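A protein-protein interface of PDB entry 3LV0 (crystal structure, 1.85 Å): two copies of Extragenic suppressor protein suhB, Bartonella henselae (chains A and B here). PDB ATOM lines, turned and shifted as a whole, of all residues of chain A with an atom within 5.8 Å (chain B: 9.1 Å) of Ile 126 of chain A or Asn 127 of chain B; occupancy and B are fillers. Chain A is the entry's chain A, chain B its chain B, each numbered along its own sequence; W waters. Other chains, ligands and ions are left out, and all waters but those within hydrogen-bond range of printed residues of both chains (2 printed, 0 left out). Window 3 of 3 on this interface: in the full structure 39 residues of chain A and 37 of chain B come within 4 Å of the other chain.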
ATOM      1  N   ARG A  23       5.835  12.692 -18.130  1.00  0.00           N
ATOM      2  CA  ARG A  23       4.616  13.429 -18.545  1.00  0.00           C
ATOM      3  C   ARG A  23       4.039  12.883 -19.862  1.00  0.00           C
ATOM      4  O   ARG A  23       2.834  12.660 -19.989  1.00  0.00           O
ATOM      5  CB  ARG A  23       4.880  14.952 -18.668  1.00  0.00           C
ATOM      6  CG  ARG A  23       5.350  15.632 -17.351  1.00  0.00           C
ATOM      7  CD  ARG A  23       4.347  15.505 -16.219  1.00  0.00           C
ATOM      8  NE  ARG A  23       4.640  14.371 -15.336  1.00  0.00           N
ATOM      9  CZ  ARG A  23       3.728  13.701 -14.627  1.00  0.00           C
ATOM     10  NH1 ARG A  23       2.434  14.032 -14.676  1.00  0.00           N
ATOM     11  NH2 ARG A  23       4.109  12.690 -13.863  1.00  0.00           N
ATOM     12  N   VAL A  26       2.360   9.490 -19.156  1.00  0.00           N
ATOM     13  CA  VAL A  26       1.035   9.640 -18.515  1.00  0.00           C
ATOM     14  C   VAL A  26      -0.044  10.035 -19.526  1.00  0.00           C
ATOM     15  O   VAL A  26      -1.164   9.507 -19.481  1.00  0.00           O
ATOM     16  CB  VAL A  26       1.085  10.568 -17.273  1.00  0.00           C
ATOM     17  CG1 VAL A  26      -0.343  10.909 -16.745  1.00  0.00           C
ATOM     18  CG2 VAL A  26       1.883   9.873 -16.178  1.00  0.00           C
ATOM     19  N   TYR A  29      -0.739   6.899 -21.631  1.00  0.00           N
ATOM     20  CA  TYR A  29      -1.387   5.907 -20.759  1.00  0.00           C
ATOM     21  C   TYR A  29      -2.933   6.034 -20.802  1.00  0.00           C
ATOM     22  O   TYR A  29      -3.651   5.052 -20.630  1.00  0.00           O
ATOM     23  CB  TYR A  29      -0.819   6.052 -19.336  1.00  0.00           C
ATOM     24  CG  TYR A  29      -1.405   5.138 -18.258  1.00  0.00           C
ATOM     25  CD1 TYR A  29      -1.015   3.796 -18.137  1.00  0.00           C
ATOM     26  CD2 TYR A  29      -2.296   5.647 -17.325  1.00  0.00           C
ATOM     27  CE1 TYR A  29      -1.541   2.989 -17.113  1.00  0.00           C
ATOM     28  CE2 TYR A  29      -2.826   4.858 -16.315  1.00  0.00           C
ATOM     29  CZ  TYR A  29      -2.452   3.537 -16.208  1.00  0.00           C
ATOM     30  OH  TYR A  29      -3.032   2.799 -15.190  1.00  0.00           O
ATOM     31  N   PRO A 103      -0.686   0.634 -13.188  1.00  0.00           N
ATOM     32  CA  PRO A 103       0.110   1.848 -12.770  1.00  0.00           C
ATOM     33  C   PRO A 103       1.490   1.665 -12.186  1.00  0.00           C
ATOM     34  O   PRO A 103       1.924   2.501 -11.379  1.00  0.00           O
ATOM     35  CB  PRO A 103      -0.748   2.467 -11.646  1.00  0.00           C
ATOM     36  CG  PRO A 103      -1.570   1.287 -11.085  1.00  0.00           C
ATOM     37  CD  PRO A 103      -1.901   0.457 -12.347  1.00  0.00           C
ATOM     38  N   PHE A 104       2.167   0.568 -12.477  1.00  0.00           N
ATOM     39  CA  PHE A 104       3.520   0.333 -11.970  1.00  0.00           C
ATOM     40  C   PHE A 104       4.423   0.389 -13.205  1.00  0.00           C
ATOM     41  O   PHE A 104       4.501  -0.597 -13.921  1.00  0.00           O
ATOM     42  CB  PHE A 104       3.730  -1.071 -11.304  1.00  0.00           C
ATOM     43  CG  PHE A 104       3.111  -1.246  -9.913  1.00  0.00           C
ATOM     44  CD1 PHE A 104       3.866  -1.050  -8.762  1.00  0.00           C
ATOM     45  CD2 PHE A 104       1.805  -1.714  -9.775  1.00  0.00           C
ATOM     46  CE1 PHE A 104       3.299  -1.231  -7.507  1.00  0.00           C
ATOM     47  CE2 PHE A 104       1.235  -1.900  -8.533  1.00  0.00           C
ATOM     48  CZ  PHE A 104       1.974  -1.659  -7.398  1.00  0.00           C
ATOM     49  N   PHE A 105       5.092   1.520 -13.437  1.00  0.00           N
ATOM     50  CA  PHE A 105       6.061   1.582 -14.540  1.00  0.00           C
ATOM     51  C   PHE A 105       6.885   2.837 -14.304  1.00  0.00           C
ATOM     52  O   PHE A 105       6.475   3.687 -13.486  1.00  0.00           O
ATOM     53  CB  PHE A 105       5.358   1.541 -15.932  1.00  0.00           C
ATOM     54  CG  PHE A 105       4.362   2.631 -16.161  1.00  0.00           C
ATOM     55  CD1 PHE A 105       4.776   3.938 -16.515  1.00  0.00           C
ATOM     56  CD2 PHE A 105       2.989   2.376 -16.025  1.00  0.00           C
ATOM     57  CE1 PHE A 105       3.841   4.938 -16.713  1.00  0.00           C
ATOM     58  CE2 PHE A 105       2.042   3.395 -16.247  1.00  0.00           C
ATOM     59  CZ  PHE A 105       2.477   4.670 -16.582  1.00  0.00           C
ATOM     60  N   ASN A 124       8.596   7.152 -11.433  1.00  0.00           N
ATOM     61  CA  ASN A 124       7.279   6.592 -11.718  1.00  0.00           C
ATOM     62  C   ASN A 124       6.313   7.770 -11.850  1.00  0.00           C
ATOM     63  O   ASN A 124       5.999   8.432 -10.865  1.00  0.00           O
ATOM     64  CB  ASN A 124       6.825   5.652 -10.576  1.00  0.00           C
ATOM     65  CG  ASN A 124       5.359   5.205 -10.722  1.00  0.00           C
ATOM     66  OD1 ASN A 124       4.607   5.724 -11.532  1.00  0.00           O
ATOM     67  ND2 ASN A 124       4.956   4.256  -9.902  1.00  0.00           N
ATOM     68  N   PRO A 125       5.857   8.063 -13.077  1.00  0.00           N
ATOM     69  CA  PRO A 125       5.114   9.308 -13.260  1.00  0.00           C
ATOM     70  C   PRO A 125       3.644   9.217 -12.835  1.00  0.00           C
ATOM     71  O   PRO A 125       3.006  10.242 -12.635  1.00  0.00           O
ATOM     72  CB  PRO A 125       5.243   9.565 -14.769  1.00  0.00           C
ATOM     73  CG  PRO A 125       5.272   8.153 -15.346  1.00  0.00           C
ATOM     74  CD  PRO A 125       6.104   7.358 -14.360  1.00  0.00           C
ATOM     75  N   ILE A 126       3.108   8.005 -12.724  1.00  0.00           N
ATOM     76  CA  ILE A 126       1.716   7.817 -12.271  1.00  0.00           C
ATOM     77  C   ILE A 126       1.587   8.297 -10.840  1.00  0.00           C
ATOM     78  O   ILE A 126       0.672   9.037 -10.503  1.00  0.00           O
ATOM     79  CB  ILE A 126       1.301   6.299 -12.308  1.00  0.00           C
ATOM     80  CG1 ILE A 126       1.003   5.895 -13.744  1.00  0.00           C
ATOM     81  CG2 ILE A 126       0.057   6.025 -11.377  1.00  0.00           C
ATOM     82  CD1 ILE A 126      -0.254   6.528 -14.302  1.00  0.00           C
ATOM     83  N   ASN A 127       2.503   7.850  -9.998  1.00  0.00           N
ATOM     84  CA  ASN A 127       2.484   8.193  -8.572  1.00  0.00           C
ATOM     85  C   ASN A 127       3.393   9.380  -8.238  1.00  0.00           C
ATOM     86  O   ASN A 127       3.528   9.760  -7.056  1.00  0.00           O
ATOM     87  CB  ASN A 127       2.873   6.951  -7.742  1.00  0.00           C
ATOM     88  CG  ASN A 127       1.883   5.812  -7.920  1.00  0.00           C
ATOM     89  OD1 ASN A 127       0.683   6.039  -7.978  1.00  0.00           O
ATOM     90  ND2 ASN A 127       2.374   4.605  -8.015  1.00  0.00           N
ATOM     91  N   ASP A 128       4.025   9.941  -9.271  1.00  0.00           N
ATOM     92  CA  ASP A 128       4.998  11.046  -9.136  1.00  0.00           C
ATOM     93  C   ASP A 128       6.068  10.675  -8.088  1.00  0.00           C
ATOM     94  O   ASP A 128       6.303  11.420  -7.123  1.00  0.00           O
ATOM     95  CB  ASP A 128       4.254  12.367  -8.781  1.00  0.00           C
ATOM     96  CG  ASP A 128       5.139  13.613  -8.874  1.00  0.00           C
ATOM     97  OD1 ASP A 128       6.069  13.711  -9.711  1.00  0.00           O
ATOM     98  OD2 ASP A 128       4.868  14.556  -8.103  1.00  0.00           O
ATOM     99  N   GLY B  22     -11.007   5.856   2.415  1.00  0.00           N
ATOM    100  CA  GLY B  22      -9.838   5.958   1.540  1.00  0.00           C
ATOM    101  C   GLY B  22      -8.992   7.197   1.818  1.00  0.00           C
ATOM    102  O   GLY B  22      -7.759   7.121   1.830  1.00  0.00           O
ATOM    103  N   VAL B  26      -5.114   7.441   2.991  1.00  0.00           N
ATOM    104  CA  VAL B  26      -4.107   8.293   2.301  1.00  0.00           C
ATOM    105  C   VAL B  26      -3.388   9.220   3.273  1.00  0.00           C
ATOM    106  O   VAL B  26      -2.170   9.406   3.167  1.00  0.00           O
ATOM    107  CB  VAL B  26      -4.706   9.091   1.087  1.00  0.00           C
ATOM    108  CG1 VAL B  26      -3.693  10.143   0.551  1.00  0.00           C
ATOM    109  CG2 VAL B  26      -5.027   8.130  -0.025  1.00  0.00           C
ATOM    110  N   TYR B  29      -1.080   6.916   5.185  1.00  0.00           N
ATOM    111  CA  TYR B  29      -0.022   6.424   4.325  1.00  0.00           C
ATOM    112  C   TYR B  29       1.184   7.390   4.223  1.00  0.00           C
ATOM    113  O   TYR B  29       2.334   6.951   4.233  1.00  0.00           O
ATOM    114  CB  TYR B  29      -0.591   6.124   2.946  1.00  0.00           C
ATOM    115  CG  TYR B  29       0.413   5.673   1.908  1.00  0.00           C
ATOM    116  CD1 TYR B  29       0.770   4.328   1.783  1.00  0.00           C
ATOM    117  CD2 TYR B  29       0.993   6.597   1.045  1.00  0.00           C
ATOM    118  CE1 TYR B  29       1.690   3.917   0.803  1.00  0.00           C
ATOM    119  CE2 TYR B  29       1.906   6.210   0.092  1.00  0.00           C
ATOM    120  CZ  TYR B  29       2.261   4.882  -0.028  1.00  0.00           C
ATOM    121  OH  TYR B  29       3.182   4.566  -1.009  1.00  0.00           O
ATOM    122  N   ILE B 102       3.934   0.394  -0.069  1.00  0.00           N
ATOM    123  CA  ILE B 102       3.648  -0.013  -1.448  1.00  0.00           C
ATOM    124  C   ILE B 102       2.280   0.535  -1.830  1.00  0.00           C
ATOM    125  O   ILE B 102       1.244   0.158  -1.240  1.00  0.00           O
ATOM    126  CB  ILE B 102       3.715  -1.553  -1.651  1.00  0.00           C
ATOM    127  CG1 ILE B 102       5.150  -2.070  -1.409  1.00  0.00           C
ATOM    128  CG2 ILE B 102       3.189  -1.942  -3.045  1.00  0.00           C
ATOM    129  CD1 ILE B 102       5.200  -3.613  -1.195  1.00  0.00           C
ATOM    130  N   PRO B 103       2.264   1.424  -2.839  1.00  0.00           N
ATOM    131  CA  PRO B 103       1.122   2.334  -2.938  1.00  0.00           C
ATOM    132  C   PRO B 103       0.085   1.645  -3.737  1.00  0.00           C
ATOM    133  O   PRO B 103      -0.248   2.122  -4.817  1.00  0.00           O
ATOM    134  CB  PRO B 103       1.700   3.535  -3.710  1.00  0.00           C
ATOM    135  CG  PRO B 103       2.768   2.904  -4.580  1.00  0.00           C
ATOM    136  CD  PRO B 103       3.358   1.787  -3.762  1.00  0.00           C
ATOM    137  N   PHE B 104      -0.362   0.484  -3.237  1.00  0.00           N
ATOM    138  CA  PHE B 104      -1.285  -0.397  -3.902  1.00  0.00           C
ATOM    139  C   PHE B 104      -2.171  -1.179  -2.907  1.00  0.00           C
ATOM    140  O   PHE B 104      -1.793  -2.233  -2.355  1.00  0.00           O
ATOM    141  CB  PHE B 104      -0.574  -1.358  -4.833  1.00  0.00           C
ATOM    142  CG  PHE B 104      -1.431  -1.819  -5.971  1.00  0.00           C
ATOM    143  CD1 PHE B 104      -1.765  -0.941  -7.006  1.00  0.00           C
ATOM    144  CD2 PHE B 104      -1.962  -3.100  -5.978  1.00  0.00           C
ATOM    145  CE1 PHE B 104      -2.592  -1.361  -8.061  1.00  0.00           C
ATOM    146  CE2 PHE B 104      -2.778  -3.538  -7.036  1.00  0.00           C
ATOM    147  CZ  PHE B 104      -3.091  -2.662  -8.078  1.00  0.00           C
ATOM    148  N   PHE B 105      -3.373  -0.649  -2.697  1.00  0.00           N
ATOM    149  CA  PHE B 105      -4.257  -1.189  -1.664  1.00  0.00           C
ATOM    150  C   PHE B 105      -5.611  -0.538  -1.860  1.00  0.00           C
ATOM    151  O   PHE B 105      -5.735   0.406  -2.665  1.00  0.00           O
ATOM    152  CB  PHE B 105      -3.702  -0.896  -0.253  1.00  0.00           C
ATOM    153  CG  PHE B 105      -3.353   0.543  -0.014  1.00  0.00           C
ATOM    154  CD1 PHE B 105      -4.347   1.469   0.387  1.00  0.00           C
ATOM    155  CD2 PHE B 105      -2.015   0.980  -0.132  1.00  0.00           C
ATOM    156  CE1 PHE B 105      -4.015   2.804   0.622  1.00  0.00           C
ATOM    157  CE2 PHE B 105      -1.672   2.307   0.127  1.00  0.00           C
ATOM    158  CZ  PHE B 105      -2.683   3.228   0.488  1.00  0.00           C
ATOM    159  N   ALA B 106      -6.638  -1.015  -1.143  1.00  0.00           N
ATOM    160  CA  ALA B 106      -7.990  -0.579  -1.487  1.00  0.00           C
ATOM    161  C   ALA B 106      -8.940  -0.758  -0.319  1.00  0.00           C
ATOM    162  O   ALA B 106      -8.643  -1.476   0.636  1.00  0.00           O
ATOM    163  CB  ALA B 106      -8.530  -1.386  -2.706  1.00  0.00           C
ATOM    164  N   TYR B 123     -12.261   0.764  -3.838  1.00  0.00           N
ATOM    165  CA  TYR B 123     -11.642   2.058  -4.027  1.00  0.00           C
ATOM    166  C   TYR B 123     -10.161   2.036  -3.670  1.00  0.00           C
ATOM    167  O   TYR B 123      -9.788   1.777  -2.527  1.00  0.00           O
ATOM    168  CB  TYR B 123     -12.396   3.113  -3.190  1.00  0.00           C
ATOM    169  CG  TYR B 123     -11.844   4.516  -3.336  1.00  0.00           C
ATOM    170  CD1 TYR B 123     -11.733   5.117  -4.595  1.00  0.00           C
ATOM    171  CD2 TYR B 123     -11.444   5.238  -2.224  1.00  0.00           C
ATOM    172  CE1 TYR B 123     -11.204   6.415  -4.733  1.00  0.00           C
ATOM    173  CE2 TYR B 123     -10.947   6.550  -2.346  1.00  0.00           C
ATOM    174  CZ  TYR B 123     -10.821   7.117  -3.593  1.00  0.00           C
ATOM    175  OH  TYR B 123     -10.334   8.397  -3.714  1.00  0.00           O
ATOM    176  N   ASN B 124      -9.339   2.349  -4.662  1.00  0.00           N
ATOM    177  CA  ASN B 124      -7.897   2.549  -4.478  1.00  0.00           C
ATOM    178  C   ASN B 124      -7.650   4.041  -4.311  1.00  0.00           C
ATOM    179  O   ASN B 124      -7.702   4.798  -5.275  1.00  0.00           O
ATOM    180  CB  ASN B 124      -7.167   2.004  -5.684  1.00  0.00           C
ATOM    181  CG  ASN B 124      -5.705   2.377  -5.713  1.00  0.00           C
ATOM    182  OD1 ASN B 124      -5.188   3.049  -4.826  1.00  0.00           O
ATOM    183  ND2 ASN B 124      -5.030   1.948  -6.775  1.00  0.00           N
ATOM    184  N   PRO B 125      -7.397   4.473  -3.077  1.00  0.00           N
ATOM    185  CA  PRO B 125      -7.350   5.901  -2.840  1.00  0.00           C
ATOM    186  C   PRO B 125      -6.031   6.549  -3.259  1.00  0.00           C
ATOM    187  O   PRO B 125      -5.993   7.760  -3.420  1.00  0.00           O
ATOM    188  CB  PRO B 125      -7.555   6.000  -1.330  1.00  0.00           C
ATOM    189  CG  PRO B 125      -6.841   4.801  -0.835  1.00  0.00           C
ATOM    190  CD  PRO B 125      -7.193   3.710  -1.825  1.00  0.00           C
ATOM    191  N   ILE B 126      -4.986   5.752  -3.435  1.00  0.00           N
ATOM    192  CA  ILE B 126      -3.709   6.249  -3.960  1.00  0.00           C
ATOM    193  C   ILE B 126      -3.838   6.747  -5.384  1.00  0.00           C
ATOM    194  O   ILE B 126      -3.373   7.846  -5.714  1.00  0.00           O
ATOM    195  CB  ILE B 126      -2.581   5.171  -3.915  1.00  0.00           C
ATOM    196  CG1 ILE B 126      -2.180   4.908  -2.465  1.00  0.00           C
ATOM    197  CG2 ILE B 126      -1.305   5.646  -4.738  1.00  0.00           C
ATOM    198  CD1 ILE B 126      -1.558   6.156  -1.722  1.00  0.00           C
ATOM    199  N   ASN B 127      -4.458   5.956  -6.238  1.00  0.00           N
ATOM    200  CA  ASN B 127      -4.605   6.351  -7.645  1.00  0.00           C
ATOM    201  C   ASN B 127      -5.992   6.906  -7.935  1.00  0.00           C
ATOM    202  O   ASN B 127      -6.298   7.232  -9.081  1.00  0.00           O
ATOM    203  CB  ASN B 127      -4.339   5.149  -8.556  1.00  0.00           C
ATOM    204  CG  ASN B 127      -2.916   4.649  -8.450  1.00  0.00           C
ATOM    205  OD1 ASN B 127      -2.678   3.456  -8.234  1.00  0.00           O
ATOM    206  ND2 ASN B 127      -1.954   5.565  -8.609  1.00  0.00           N
ATOM    207  N   ASP B 128      -6.812   7.038  -6.892  1.00  0.00           N
ATOM    208  CA  ASP B 128      -8.188   7.549  -7.017  1.00  0.00           C
ATOM    209  C   ASP B 128      -8.955   6.729  -8.066  1.00  0.00           C
ATOM    210  O   ASP B 128      -9.548   7.279  -9.007  1.00  0.00           O
ATOM    211  CB  ASP B 128      -8.222   9.078  -7.325  1.00  0.00           C
ATOM    212  CG  ASP B 128      -9.620   9.683  -7.184  1.00  0.00           C
ATOM    213  OD1 ASP B 128     -10.406   9.269  -6.305  1.00  0.00           O
ATOM    214  OD2 ASP B 128      -9.934  10.618  -7.950  1.00  0.00           O
ATOM    215  N   GLU B 129      -8.929   5.414  -7.897  1.00  0.00           N
ATOM    216  CA  GLU B 129      -9.611   4.512  -8.808  1.00  0.00           C
ATOM    217  C   GLU B 129     -10.809   3.912  -8.089  1.00  0.00           C
ATOM    218  O   GLU B 129     -10.635   3.180  -7.102  1.00  0.00           O
ATOM    219  CB  GLU B 129      -8.669   3.389  -9.253  1.00  0.00           C
ATOM    220  CG  GLU B 129      -7.451   3.939 -10.043  1.00  0.00           C
ATOM    221  CD  GLU B 129      -6.502   2.862 -10.468  1.00  0.00           C
ATOM    222  OE1 GLU B 129      -6.425   1.826  -9.807  1.00  0.00           O
ATOM    223  OE2 GLU B 129      -5.807   3.063 -11.478  1.00  0.00           O
ATOM    224  N   LEU B 130     -11.998   4.224  -8.604  1.00  0.00           N
ATOM    225  CA  LEU B 130     -13.259   3.838  -7.981  1.00  0.00           C
ATOM    226  C   LEU B 130     -13.963   2.829  -8.894  1.00  0.00           C
ATOM    227  O   LEU B 130     -14.306   3.146 -10.028  1.00  0.00           O
ATOM    228  CB  LEU B 130     -14.158   5.076  -7.791  1.00  0.00           C
ATOM    229  CG  LEU B 130     -15.536   4.792  -7.173  1.00  0.00           C
ATOM    230  CD1 LEU B 130     -15.340   4.215  -5.787  1.00  0.00           C
ATOM    231  CD2 LEU B 130     -16.409   6.089  -7.094  1.00  0.00           C
ATOM    232  N   PHE B 131     -14.127   1.610  -8.414  1.00  0.00           N
ATOM    233  CA  PHE B 131     -14.774   0.566  -9.191  1.00  0.00           C
ATOM    234  C   PHE B 131     -16.102   0.269  -8.514  1.00  0.00           C
ATOM    235  O   PHE B 131     -16.154   0.077  -7.280  1.00  0.00           O
ATOM    236  CB  PHE B 131     -13.912  -0.697  -9.175  1.00  0.00           C
ATOM    237  CG  PHE B 131     -12.528  -0.480  -9.698  1.00  0.00           C
ATOM    238  CD1 PHE B 131     -12.271  -0.632 -11.052  1.00  0.00           C
ATOM    239  CD2 PHE B 131     -11.483  -0.103  -8.842  1.00  0.00           C
ATOM    240  CE1 PHE B 131     -10.987  -0.442 -11.569  1.00  0.00           C
ATOM    241  CE2 PHE B 131     -10.189   0.116  -9.357  1.00  0.00           C
ATOM    242  CZ  PHE B 131      -9.947  -0.078 -10.720  1.00  0.00           C
ATOM    243  N   PHE B 141     -15.787   2.060 -13.908  1.00  0.00           N
ATOM    244  CA  PHE B 141     -14.538   2.565 -13.398  1.00  0.00           C
ATOM    245  C   PHE B 141     -14.604   4.087 -13.478  1.00  0.00           C
ATOM    246  O   PHE B 141     -14.801   4.646 -14.577  1.00  0.00           O
ATOM    247  CB  PHE B 141     -13.348   2.025 -14.203  1.00  0.00           C
ATOM    248  CG  PHE B 141     -12.085   2.794 -13.967  1.00  0.00           C
ATOM    249  CD1 PHE B 141     -11.456   2.751 -12.732  1.00  0.00           C
ATOM    250  CD2 PHE B 141     -11.582   3.651 -14.956  1.00  0.00           C
ATOM    251  CE1 PHE B 141     -10.276   3.476 -12.505  1.00  0.00           C
ATOM    252  CE2 PHE B 141     -10.430   4.400 -14.735  1.00  0.00           C
ATOM    253  CZ  PHE B 141      -9.780   4.317 -13.494  1.00  0.00           C
ATOM    254  N   ASN B 142     -14.487   4.756 -12.326  1.00  0.00           N
ATOM    255  CA  ASN B 142     -14.618   6.230 -12.279  1.00  0.00           C
ATOM    256  C   ASN B 142     -15.774   6.743 -13.126  1.00  0.00           C
ATOM    257  O   ASN B 142     -15.583   7.597 -13.999  1.00  0.00           O
ATOM    258  CB  ASN B 142     -13.295   6.899 -12.713  1.00  0.00           C
ATOM    259  CG  ASN B 142     -12.205   6.747 -11.667  1.00  0.00           C
ATOM    260  OD1 ASN B 142     -12.439   6.144 -10.640  1.00  0.00           O
ATOM    261  ND2 ASN B 142     -11.013   7.295 -11.927  1.00  0.00           N
ATOM    262  N   LEU B 196      -8.605  -5.575  -5.048  1.00  0.00           N
ATOM    263  CA  LEU B 196      -8.182  -4.694  -6.130  1.00  0.00           C
ATOM    264  C   LEU B 196      -7.814  -5.523  -7.350  1.00  0.00           C
ATOM    265  O   LEU B 196      -7.996  -5.075  -8.472  1.00  0.00           O
ATOM    266  CB  LEU B 196      -6.999  -3.805  -5.691  1.00  0.00           C
ATOM    267  CG  LEU B 196      -6.609  -2.636  -6.573  1.00  0.00           C
ATOM    268  CD1 LEU B 196      -7.813  -1.706  -6.900  1.00  0.00           C
ATOM    269  CD2 LEU B 196      -5.517  -1.830  -5.863  1.00  0.00           C
ATOM    270  N   TYR B 200      -9.251  -5.091 -11.041  1.00  0.00           N
ATOM    271  CA  TYR B 200      -8.416  -4.991 -12.228  1.00  0.00           C
ATOM    272  C   TYR B 200      -8.855  -5.971 -13.336  1.00  0.00           C
ATOM    273  O   TYR B 200      -8.784  -5.642 -14.542  1.00  0.00           O
ATOM    274  CB  TYR B 200      -6.932  -5.165 -11.858  1.00  0.00           C
ATOM    275  CG  TYR B 200      -6.295  -3.828 -11.526  1.00  0.00           C
ATOM    276  CD1 TYR B 200      -6.997  -2.875 -10.769  1.00  0.00           C
ATOM    277  CD2 TYR B 200      -5.012  -3.502 -11.985  1.00  0.00           C
ATOM    278  CE1 TYR B 200      -6.451  -1.629 -10.465  1.00  0.00           C
ATOM    279  CE2 TYR B 200      -4.448  -2.253 -11.693  1.00  0.00           C
ATOM    280  CZ  TYR B 200      -5.172  -1.327 -10.923  1.00  0.00           C
ATOM    281  OH  TYR B 200      -4.660  -0.078 -10.637  1.00  0.00           O
ATOM    282  N   ARG B 205      -7.775  -4.686 -16.897  1.00  0.00           N
ATOM    283  CA  ARG B 205      -6.355  -4.378 -16.733  1.00  0.00           C
ATOM    284  C   ARG B 205      -5.522  -5.648 -16.630  1.00  0.00           C
ATOM    285  O   ARG B 205      -4.377  -5.659 -17.045  1.00  0.00           O
ATOM    286  CB  ARG B 205      -6.139  -3.500 -15.516  1.00  0.00           C
ATOM    287  CG  ARG B 205      -6.731  -2.121 -15.782  1.00  0.00           C
ATOM    288  CD  ARG B 205      -6.561  -1.301 -14.576  1.00  0.00           C
ATOM    289  NE  ARG B 205      -6.927   0.080 -14.866  1.00  0.00           N
ATOM    290  CZ  ARG B 205      -6.567   1.081 -14.080  1.00  0.00           C
ATOM    291  NH1 ARG B 205      -5.881   0.820 -12.993  1.00  0.00           N
ATOM    292  NH2 ARG B 205      -6.910   2.332 -14.371  1.00  0.00           N
HETATM  293  O   HOH W   1      -2.346   8.183  -9.527  1.00  0.00           O
HETATM  294  O   HOH W   2       0.005   2.867  -8.046  1.00  0.00           O
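OD1 of Asn 124 of chain A sits at hydrogen-bond distance from N of Ile 126 of chain A (3.0 Å).
The side-chain amide nitrogen (ND2) of Asn 124 of chain A sits close to the side-chain amide nitrogen (ND2) of Asn 127 of chain A, at 3.2 Å.
The side-chain amide oxygen (OD1) of Asn 124 of chain B lies within hydrogen-bond range of the backbone NH (N) of Ile 126 of chain B.
The side-chain carboxylate of Glu 129 of chain B sits at hydrogen-bond distance from the side-chain hydroxyl of Tyr 200 of chain B (2.7 Å).
The side-chain carboxylate (OE2) of Glu 129 of chain B is in salt-bridge range of the guanidinium group (NH1) of Arg 205 of chain B, 2.7 Å away.
O of Tyr 200 of chain B lies within hydrogen-bond range of N of Arg 205 of chain B (2.7 Å).
Val 26 of chain A touches none of the printed residues of chain B.
Of the printed residues of chain B, Pro 103 of chain A touches Asn 127 (3.7 Å) and Tyr 200 (3.3 Å).
No residue of chain B comes within 4 Å of Pro 125 of chain A.
Asn 127 of chain A touches three residues of chain B.
Asn 127 of chain B touches three residues of chain A.
Of the printed residues of chain A, Tyr 200 of chain B touches Pro 103.
Printed residues of chain A within 4 Å of Arg 205 of chain B: Tyr 29 (3.99 Å).
The nearest printed residue of chain A that does not touch Phe 104 of chain B is Pro 103 of chain A (4.1 Å).
Of the 22 printed residues of chain B, 6 touch a printed residue of chain A.
Hydrophobic or aromatic side chains of chain B within 4 Å of the printed part of chain A: Pro 103, Phe 104, Ile 126 and Tyr 200.
Hydrophobic or aromatic side chains of chain A within 4 Å of the printed part of chain B: Tyr 29, Pro 103, Phe 104 and Ile 126.
Among the printed residues, no Asp or Glu carboxylate lies within 4 Å of a Lys or Arg side-chain nitrogen of the other chain.
Water W2 lies within hydrogen-bond range of OD1 of Asn 127 of chain B (2.8 Å), ND2 of Asn 127 of chain A (2.9 Å) and O of Pro 103 of chain B (3.3 Å).
Water W1 bridges the side-chain amide nitrogen (ND2) of Asn 127 of chain B and the backbone carbonyl oxygen (O) of Ile 126 of chain A.
Tyr 29 of chain A touches Arg 205 of chain B (OH to NH2, 3.99 Å).
OD1 of Asn 127 of chain B touches CG of Pro 103 of chain A, 3.7 Å away.
Pro 103 of chain A touches Tyr 200 of chain B.
Phe 104 of chain A touches Phe 104 of chain B.
ND2 of Asn 127 of chain B touches CG2 of Ile 126 of chain A, 3.5 Å away.
CG of Pro 103 of chain B touches ND2 of Asn 127 of chain A, at 3.9 Å.
CG2 of Ile 126 of chain B touches OD1 of Asn 127 of chain A (3.8 Å).
The side-chain amide nitrogen (ND2) of Asn 127 of chain B lies within hydrogen-bond range of the side-chain amide oxygen (OD1) of Asn 127 of chain A, 2.8 Å away.
Pro 103 of chain A touches Asn 127 of chain B, and with the chains exchanged Asn 127 of chain A touches Pro 103 of chain B.
Phe 104 of chain A touches its own counterpart, Phe 104 of chain B.
Ile 126 of chain A touches Asn 127 of chain B, and with the chains exchanged Asn 127 of chain A touches Ile 126 of chain B.
Asn 127 of chain A touches its own counterpart, Asn 127 of chain B.
10 positions are printed for both chains.
Of the 8 pairs that touch across the chains among the printed residues, 6 have their exchanged pair printed and touching as well.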
